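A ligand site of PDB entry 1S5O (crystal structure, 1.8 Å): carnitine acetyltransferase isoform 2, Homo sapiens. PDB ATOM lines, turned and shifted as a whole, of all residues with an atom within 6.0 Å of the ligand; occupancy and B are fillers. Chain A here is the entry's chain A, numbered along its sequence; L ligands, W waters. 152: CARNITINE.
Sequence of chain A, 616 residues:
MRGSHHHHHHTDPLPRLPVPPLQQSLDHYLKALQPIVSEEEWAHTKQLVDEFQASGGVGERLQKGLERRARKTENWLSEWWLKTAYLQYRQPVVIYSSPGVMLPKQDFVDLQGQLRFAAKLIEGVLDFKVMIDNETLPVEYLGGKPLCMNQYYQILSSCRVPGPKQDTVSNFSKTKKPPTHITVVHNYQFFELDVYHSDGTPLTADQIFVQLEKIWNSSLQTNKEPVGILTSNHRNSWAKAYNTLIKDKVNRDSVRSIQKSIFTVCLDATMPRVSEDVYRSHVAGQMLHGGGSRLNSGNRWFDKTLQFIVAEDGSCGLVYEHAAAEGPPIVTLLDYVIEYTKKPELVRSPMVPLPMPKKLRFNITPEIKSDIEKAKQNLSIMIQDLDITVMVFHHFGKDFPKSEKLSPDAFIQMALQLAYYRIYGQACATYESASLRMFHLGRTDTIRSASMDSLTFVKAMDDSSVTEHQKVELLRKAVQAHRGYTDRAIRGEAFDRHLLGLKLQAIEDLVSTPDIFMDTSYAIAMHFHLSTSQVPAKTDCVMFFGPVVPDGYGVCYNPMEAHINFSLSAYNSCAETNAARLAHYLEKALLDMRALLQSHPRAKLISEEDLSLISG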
ATOM      1  N   TRP A  81     -28.577  34.629   6.060  1.00  0.00           N
ATOM      2  CA  TRP A  81     -28.065  33.347   5.562  1.00  0.00           C
ATOM      3  C   TRP A  81     -26.887  33.513   4.618  1.00  0.00           C
ATOM      4  O   TRP A  81     -25.901  32.778   4.691  1.00  0.00           O
ATOM      5  CB  TRP A  81     -29.216  32.594   4.907  1.00  0.00           C
ATOM      6  CG  TRP A  81     -28.830  31.253   4.397  1.00  0.00           C
ATOM      7  CD1 TRP A  81     -28.756  30.868   3.095  1.00  0.00           C
ATOM      8  CD2 TRP A  81     -28.473  30.108   5.195  1.00  0.00           C
ATOM      9  NE1 TRP A  81     -28.370  29.550   3.041  1.00  0.00           N
ATOM     10  CE2 TRP A  81     -28.190  29.065   4.311  1.00  0.00           C
ATOM     11  CE3 TRP A  81     -28.376  29.928   6.583  1.00  0.00           C
ATOM     12  CZ2 TRP A  81     -27.797  27.807   4.753  1.00  0.00           C
ATOM     13  CZ3 TRP A  81     -27.993  28.678   7.007  1.00  0.00           C
ATOM     14  CH2 TRP A  81     -27.710  27.644   6.105  1.00  0.00           C
ATOM     15  N   TYR A  86     -22.021  31.907   3.907  1.00  0.00           N
ATOM     16  CA  TYR A  86     -21.020  32.018   2.844  1.00  0.00           C
ATOM     17  C   TYR A  86     -20.071  33.183   3.039  1.00  0.00           C
ATOM     18  O   TYR A  86     -18.863  32.994   3.190  1.00  0.00           O
ATOM     19  CB  TYR A  86     -21.686  32.152   1.444  1.00  0.00           C
ATOM     20  CG  TYR A  86     -22.612  30.957   1.245  1.00  0.00           C
ATOM     21  CD1 TYR A  86     -22.069  29.686   1.163  1.00  0.00           C
ATOM     22  CD2 TYR A  86     -23.987  31.108   1.170  1.00  0.00           C
ATOM     23  CE1 TYR A  86     -22.872  28.573   0.998  1.00  0.00           C
ATOM     24  CE2 TYR A  86     -24.790  30.003   1.010  1.00  0.00           C
ATOM     25  CZ  TYR A  86     -24.238  28.747   0.924  1.00  0.00           C
ATOM     26  OH  TYR A  86     -25.041  27.642   0.763  1.00  0.00           O
ATOM     27  N   PRO A  99     -19.780  23.554  -4.672  1.00  0.00           N
ATOM     28  CA  PRO A  99     -20.055  22.215  -5.167  1.00  0.00           C
ATOM     29  C   PRO A  99     -19.728  22.052  -6.660  1.00  0.00           C
ATOM     30  O   PRO A  99     -19.814  22.929  -7.510  1.00  0.00           O
ATOM     31  CB  PRO A  99     -21.557  22.050  -4.933  1.00  0.00           C
ATOM     32  CG  PRO A  99     -22.002  23.245  -4.180  1.00  0.00           C
ATOM     33  CD  PRO A  99     -21.009  24.337  -4.467  1.00  0.00           C
ATOM     34  N   TYR A 320     -19.503  25.477  -9.121  1.00  0.00           N
ATOM     35  CA  TYR A 320     -20.206  26.755  -8.963  1.00  0.00           C
ATOM     36  C   TYR A 320     -19.936  27.372  -7.606  1.00  0.00           C
ATOM     37  O   TYR A 320     -19.811  26.670  -6.606  1.00  0.00           O
ATOM     38  CB  TYR A 320     -21.697  26.564  -9.221  1.00  0.00           C
ATOM     39  CG  TYR A 320     -22.615  26.002  -8.157  1.00  0.00           C
ATOM     40  CD1 TYR A 320     -23.151  26.803  -7.158  1.00  0.00           C
ATOM     41  CD2 TYR A 320     -22.970  24.662  -8.160  1.00  0.00           C
ATOM     42  CE1 TYR A 320     -23.993  26.282  -6.189  1.00  0.00           C
ATOM     43  CE2 TYR A 320     -23.808  24.105  -7.208  1.00  0.00           C
ATOM     44  CZ  TYR A 320     -24.307  24.940  -6.227  1.00  0.00           C
ATOM     45  OH  TYR A 320     -25.148  24.414  -5.271  1.00  0.00           O
ATOM     46  N   HIS A 322     -21.085  28.991  -4.396  1.00  0.00           N
ATOM     47  CA  HIS A 322     -22.359  28.757  -3.737  1.00  0.00           C
ATOM     48  C   HIS A 322     -23.047  29.974  -3.154  1.00  0.00           C
ATOM     49  O   HIS A 322     -24.242  29.881  -2.841  1.00  0.00           O
ATOM     50  CB  HIS A 322     -22.112  27.747  -2.591  1.00  0.00           C
ATOM     51  CG  HIS A 322     -23.290  26.862  -2.319  1.00  0.00           C
ATOM     52  ND1 HIS A 322     -24.592  27.241  -2.530  1.00  0.00           N
ATOM     53  CD2 HIS A 322     -23.347  25.589  -1.845  1.00  0.00           C
ATOM     54  CE1 HIS A 322     -25.391  26.254  -2.200  1.00  0.00           C
ATOM     55  NE2 HIS A 322     -24.674  25.229  -1.779  1.00  0.00           N
ATOM     56  N   GLU A 326     -27.913  27.838  -5.560  1.00  0.00           N
ATOM     57  CA  GLU A 326     -28.288  26.534  -5.044  1.00  0.00           C
ATOM     58  C   GLU A 326     -28.176  25.486  -6.125  1.00  0.00           C
ATOM     59  O   GLU A 326     -28.012  25.795  -7.305  1.00  0.00           O
ATOM     60  CB  GLU A 326     -29.713  26.571  -4.482  1.00  0.00           C
ATOM     61  CG  GLU A 326     -29.911  27.688  -3.465  1.00  0.00           C
ATOM     62  CD  GLU A 326     -29.076  27.430  -2.221  1.00  0.00           C
ATOM     63  OE1 GLU A 326     -28.749  26.250  -1.995  1.00  0.00           O
ATOM     64  OE2 GLU A 326     -28.752  28.390  -1.490  1.00  0.00           O
ATOM     65  N   GLY A 327     -28.195  24.237  -5.740  1.00  0.00           N
ATOM     66  CA  GLY A 327     -28.020  23.168  -6.700  1.00  0.00           C
ATOM     67  C   GLY A 327     -29.066  23.162  -7.797  1.00  0.00           C
ATOM     68  O   GLY A 327     -28.688  23.285  -8.953  1.00  0.00           O
ATOM     69  N   TYR A 431     -28.344  16.404   8.092  1.00  0.00           N
ATOM     70  CA  TYR A 431     -28.950  17.550   7.415  1.00  0.00           C
ATOM     71  C   TYR A 431     -29.403  17.099   6.035  1.00  0.00           C
ATOM     72  O   TYR A 431     -28.631  16.502   5.292  1.00  0.00           O
ATOM     73  CB  TYR A 431     -27.928  18.660   7.369  1.00  0.00           C
ATOM     74  CG  TYR A 431     -28.142  19.923   6.600  1.00  0.00           C
ATOM     75  CD1 TYR A 431     -28.183  20.013   5.222  1.00  0.00           C
ATOM     76  CD2 TYR A 431     -28.286  21.117   7.308  1.00  0.00           C
ATOM     77  CE1 TYR A 431     -28.370  21.176   4.504  1.00  0.00           C
ATOM     78  CE2 TYR A 431     -28.484  22.297   6.621  1.00  0.00           C
ATOM     79  CZ  TYR A 431     -28.521  22.321   5.243  1.00  0.00           C
ATOM     80  OH  TYR A 431     -28.720  23.514   4.573  1.00  0.00           O
ATOM     81  N   GLU A 432     -30.591  17.421   5.614  1.00  0.00           N
ATOM     82  CA  GLU A 432     -30.956  17.268   4.208  1.00  0.00           C
ATOM     83  C   GLU A 432     -31.438  18.645   3.738  1.00  0.00           C
ATOM     84  O   GLU A 432     -32.272  19.260   4.391  1.00  0.00           O
ATOM     85  CB  GLU A 432     -32.001  16.189   3.935  1.00  0.00           C
ATOM     86  CG  GLU A 432     -32.238  16.062   2.426  1.00  0.00           C
ATOM     87  CD  GLU A 432     -33.431  15.218   2.062  1.00  0.00           C
ATOM     88  OE1 GLU A 432     -34.124  14.721   2.982  1.00  0.00           O
ATOM     89  OE2 GLU A 432     -33.685  15.071   0.843  1.00  0.00           O
ATOM     90  N   SER A 433     -30.934  19.113   2.600  1.00  0.00           N
ATOM     91  CA  SER A 433     -31.372  20.427   2.153  1.00  0.00           C
ATOM     92  C   SER A 433     -32.808  20.438   1.625  1.00  0.00           C
ATOM     93  O   SER A 433     -33.209  19.567   0.839  1.00  0.00           O
ATOM     94  CB  SER A 433     -30.471  20.951   1.050  1.00  0.00           C
ATOM     95  OG  SER A 433     -29.143  20.484   1.217  1.00  0.00           O
ATOM     96  N   ALA A 434     -33.581  21.436   2.050  1.00  0.00           N
ATOM     97  CA  ALA A 434     -34.924  21.692   1.581  1.00  0.00           C
ATOM     98  C   ALA A 434     -35.035  23.054   0.878  1.00  0.00           C
ATOM     99  O   ALA A 434     -34.565  24.066   1.384  1.00  0.00           O
ATOM    100  CB  ALA A 434     -35.936  21.734   2.719  1.00  0.00           C
ATOM    101  N   THR A 444     -33.025  27.854   1.362  1.00  0.00           N
ATOM    102  CA  THR A 444     -33.116  26.504   1.900  1.00  0.00           C
ATOM    103  C   THR A 444     -33.415  26.543   3.399  1.00  0.00           C
ATOM    104  O   THR A 444     -33.307  27.575   4.063  1.00  0.00           O
ATOM    105  CB  THR A 444     -31.797  25.728   1.740  1.00  0.00           C
ATOM    106  OG1 THR A 444     -30.786  26.472   2.463  1.00  0.00           O
ATOM    107  CG2 THR A 444     -31.361  25.592   0.300  1.00  0.00           C
ATOM    108  N   ASP A 445     -33.800  25.386   3.909  1.00  0.00           N
ATOM    109  CA  ASP A 445     -33.929  25.145   5.343  1.00  0.00           C
ATOM    110  C   ASP A 445     -33.522  23.697   5.581  1.00  0.00           C
ATOM    111  O   ASP A 445     -33.210  22.947   4.649  1.00  0.00           O
ATOM    112  CB  ASP A 445     -35.348  25.383   5.836  1.00  0.00           C
ATOM    113  CG  ASP A 445     -35.426  25.703   7.317  1.00  0.00           C
ATOM    114  OD1 ASP A 445     -34.568  25.244   8.107  1.00  0.00           O
ATOM    115  OD2 ASP A 445     -36.379  26.418   7.679  1.00  0.00           O
ATOM    116  N   ARG A 497     -33.537  27.164  10.468  1.00  0.00           N
ATOM    117  CA  ARG A 497     -33.228  28.569  10.148  1.00  0.00           C
ATOM    118  C   ARG A 497     -33.921  29.458  11.173  1.00  0.00           C
ATOM    119  O   ARG A 497     -33.467  30.543  11.505  1.00  0.00           O
ATOM    120  CB  ARG A 497     -33.654  28.990   8.745  1.00  0.00           C
ATOM    121  CG  ARG A 497     -33.023  28.247   7.593  1.00  0.00           C
ATOM    122  CD  ARG A 497     -31.530  28.533   7.429  1.00  0.00           C
ATOM    123  NE  ARG A 497     -31.031  27.684   6.364  1.00  0.00           N
ATOM    124  CZ  ARG A 497     -30.747  26.400   6.453  1.00  0.00           C
ATOM    125  NH1 ARG A 497     -30.310  25.708   5.399  1.00  0.00           N
ATOM    126  NH2 ARG A 497     -30.910  25.787   7.618  1.00  0.00           N
ATOM    127  N   SER A 531     -24.042  15.334   5.906  1.00  0.00           N
ATOM    128  CA  SER A 531     -24.525  16.579   5.294  1.00  0.00           C
ATOM    129  C   SER A 531     -25.046  16.236   3.913  1.00  0.00           C
ATOM    130  O   SER A 531     -24.291  15.739   3.076  1.00  0.00           O
ATOM    131  CB  SER A 531     -23.407  17.615   5.231  1.00  0.00           C
ATOM    132  OG  SER A 531     -23.844  18.760   4.513  1.00  0.00           O
ATOM    133  N   THR A 532     -26.343  16.399   3.642  1.00  0.00           N
ATOM    134  CA  THR A 532     -26.841  15.745   2.420  1.00  0.00           C
ATOM    135  C   THR A 532     -27.733  16.676   1.594  1.00  0.00           C
ATOM    136  O   THR A 532     -28.304  17.657   2.081  1.00  0.00           O
ATOM    137  CB  THR A 532     -27.618  14.445   2.709  1.00  0.00           C
ATOM    138  OG1 THR A 532     -28.922  14.759   3.223  1.00  0.00           O
ATOM    139  CG2 THR A 532     -26.959  13.567   3.781  1.00  0.00           C
ATOM    140  N   SER A 533     -27.883  16.338   0.323  1.00  0.00           N
ATOM    141  CA  SER A 533     -28.858  17.020  -0.531  1.00  0.00           C
ATOM    142  C   SER A 533     -29.220  16.156  -1.738  1.00  0.00           C
ATOM    143  O   SER A 533     -28.389  15.444  -2.327  1.00  0.00           O
ATOM    144  CB  SER A 533     -28.317  18.396  -0.941  1.00  0.00           C
ATOM    145  OG  SER A 533     -27.774  18.314  -2.248  1.00  0.00           O
ATOM    146  N   PHE A 545     -19.797  17.653  -2.842  1.00  0.00           N
ATOM    147  CA  PHE A 545     -19.240  18.715  -2.014  1.00  0.00           C
ATOM    148  C   PHE A 545     -18.518  18.076  -0.828  1.00  0.00           C
ATOM    149  O   PHE A 545     -18.671  16.884  -0.578  1.00  0.00           O
ATOM    150  CB  PHE A 545     -20.320  19.669  -1.521  1.00  0.00           C
ATOM    151  CG  PHE A 545     -21.569  18.933  -1.040  1.00  0.00           C
ATOM    152  CD1 PHE A 545     -21.649  18.439   0.258  1.00  0.00           C
ATOM    153  CD2 PHE A 545     -22.650  18.734  -1.885  1.00  0.00           C
ATOM    154  CE1 PHE A 545     -22.782  17.769   0.689  1.00  0.00           C
ATOM    155  CE2 PHE A 545     -23.793  18.068  -1.463  1.00  0.00           C
ATOM    156  CZ  PHE A 545     -23.854  17.579  -0.174  1.00  0.00           C
ATOM    157  N   GLY A 546     -17.741  18.866  -0.096  1.00  0.00           N
ATOM    158  CA  GLY A 546     -17.011  18.254   1.013  1.00  0.00           C
ATOM    159  C   GLY A 546     -17.922  18.151   2.233  1.00  0.00           C
ATOM    160  O   GLY A 546     -18.972  18.806   2.247  1.00  0.00           O
ATOM    161  N   VAL A 548     -19.102  18.837   6.093  1.00  0.00           N
ATOM    162  CA  VAL A 548     -19.113  20.135   6.768  1.00  0.00           C
ATOM    163  C   VAL A 548     -18.440  20.037   8.140  1.00  0.00           C
ATOM    164  O   VAL A 548     -18.272  21.074   8.782  1.00  0.00           O
ATOM    165  CB  VAL A 548     -20.555  20.659   6.878  1.00  0.00           C
ATOM    166  CG1 VAL A 548     -21.230  20.645   5.506  1.00  0.00           C
ATOM    167  CG2 VAL A 548     -21.355  19.845   7.881  1.00  0.00           C
HETATM  168  C1  152 L   1     -28.062  24.396   1.606  1.00  0.00           C
HETATM  169  O1A 152 L   1     -28.163  25.537   2.086  1.00  0.00           O
HETATM  170  O1B 152 L   1     -28.616  23.356   2.034  1.00  0.00           O
HETATM  171  C2  152 L   1     -27.192  24.244   0.353  1.00  0.00           C
HETATM  172  C3  152 L   1     -26.453  22.894   0.370  1.00  0.00           C
HETATM  173  O3  152 L   1     -25.732  22.853  -0.879  1.00  0.00           O
HETATM  174  C4  152 L   1     -25.439  22.926   1.526  1.00  0.00           C
HETATM  175  N5  152 L   1     -24.836  21.528   1.713  1.00  0.00           N
HETATM  176  C5A 152 L   1     -24.027  21.103   0.486  1.00  0.00           C
HETATM  177  C5B 152 L   1     -23.894  21.591   2.931  1.00  0.00           C
HETATM  178  C5C 152 L   1     -25.934  20.514   2.009  1.00  0.00           C
HETATM  179  O   HOH W   1     -24.594  25.730   3.077  1.00  0.00           O
HETATM  180  O   HOH W   2     -27.559  27.799   0.602  1.00  0.00           O
HETATM  181  O   HOH W   3     -21.461  23.022  -0.127  1.00  0.00           O
HETATM  182  O   HOH W   4     -27.766  21.492  -2.885  1.00  0.00           O
HETATM  183  O   HOH W   5     -26.095  24.507   4.543  1.00  0.00           O
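Trp 81 touches the ligand. OH of Tyr 86 touches O1A of the ligand (3.99 Å). OE1 of Glu 326 touches C2 of the ligand, 3.5 Å away. Ser 531 touches the ligand (OG to C5B, 3.2 Å). Thr 532 touches the ligand (O to C5C, 3.7 Å). Phe 545 touches the ligand. CG1 of Val 548 touches C5B of the ligand, 3.8 Å away. Hydrophobic or aromatic side chains that line the ligand: Trp 81, His 322, Tyr 431, Phe 545 and Val 548. 12 residues have an atom within 4 Å of the ligand: Trp 81, Tyr 86, His 322, Glu 326, Tyr 431, Ser 433, Thr 444, Arg 497, Ser 531, Thr 532, Phe 545 and Val 548.
O1B of the ligand is in hydrogen-bond range of OH of Tyr 431 (2.5 Å). A ring nitrogen (NE2) of His 322 sits at hydrogen-bond distance from an oxygen (O3) of the ligand (2.8 Å). An oxygen (O1A) of the ligand sits at hydrogen-bond distance from the side-chain hydroxyl (OG1) of Thr 444 (2.8 Å). The side-chain hydroxyl of Ser 433 lies within hydrogen-bond range of an oxygen (O1B) of the ligand (3.0 Å). The guanidinium group (NH1) of Arg 497 lies within salt-bridge range of an oxygen (O1A) of the ligand.
Water W2 lies within hydrogen-bond range of OE2 of Glu 326 (2.5 Å), OH of Tyr 86 (2.5 Å), O1A of the ligand (2.8 Å) and NE1 of Trp 81 (3.1 Å). Water W4 bridges O3 of the ligand (3.2 Å) and OG of Ser 533 (3.2 Å). Water W5 lies within hydrogen-bond range of OH of Tyr 431 (2.8 Å) and O1A of the ligand (3.4 Å).
OG1 of Thr 532 sits at hydrogen-bond distance from O of Tyr 431, at 2.7 Å. The guanidinium group (NH1) of Arg 497 is in hydrogen-bond range of the side-chain hydroxyl (OH) of Tyr 431, at 2.8 Å. A ring nitrogen (ND1) of His 322 sits close to the side-chain hydroxyl (OH) of Tyr 86 (3.3 Å). The side-chain hydroxyl of Thr 444 sits at hydrogen-bond distance from the guanidinium group of Arg 497 (3.1 Å). O of Thr 532 is in hydrogen-bond range of N of Ser 433, 3.1 Å away. The side-chain carboxylate (OD1) of Asp 445 lies within salt-bridge range of the guanidinium group (NH2) of Arg 497 (3.7 Å).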
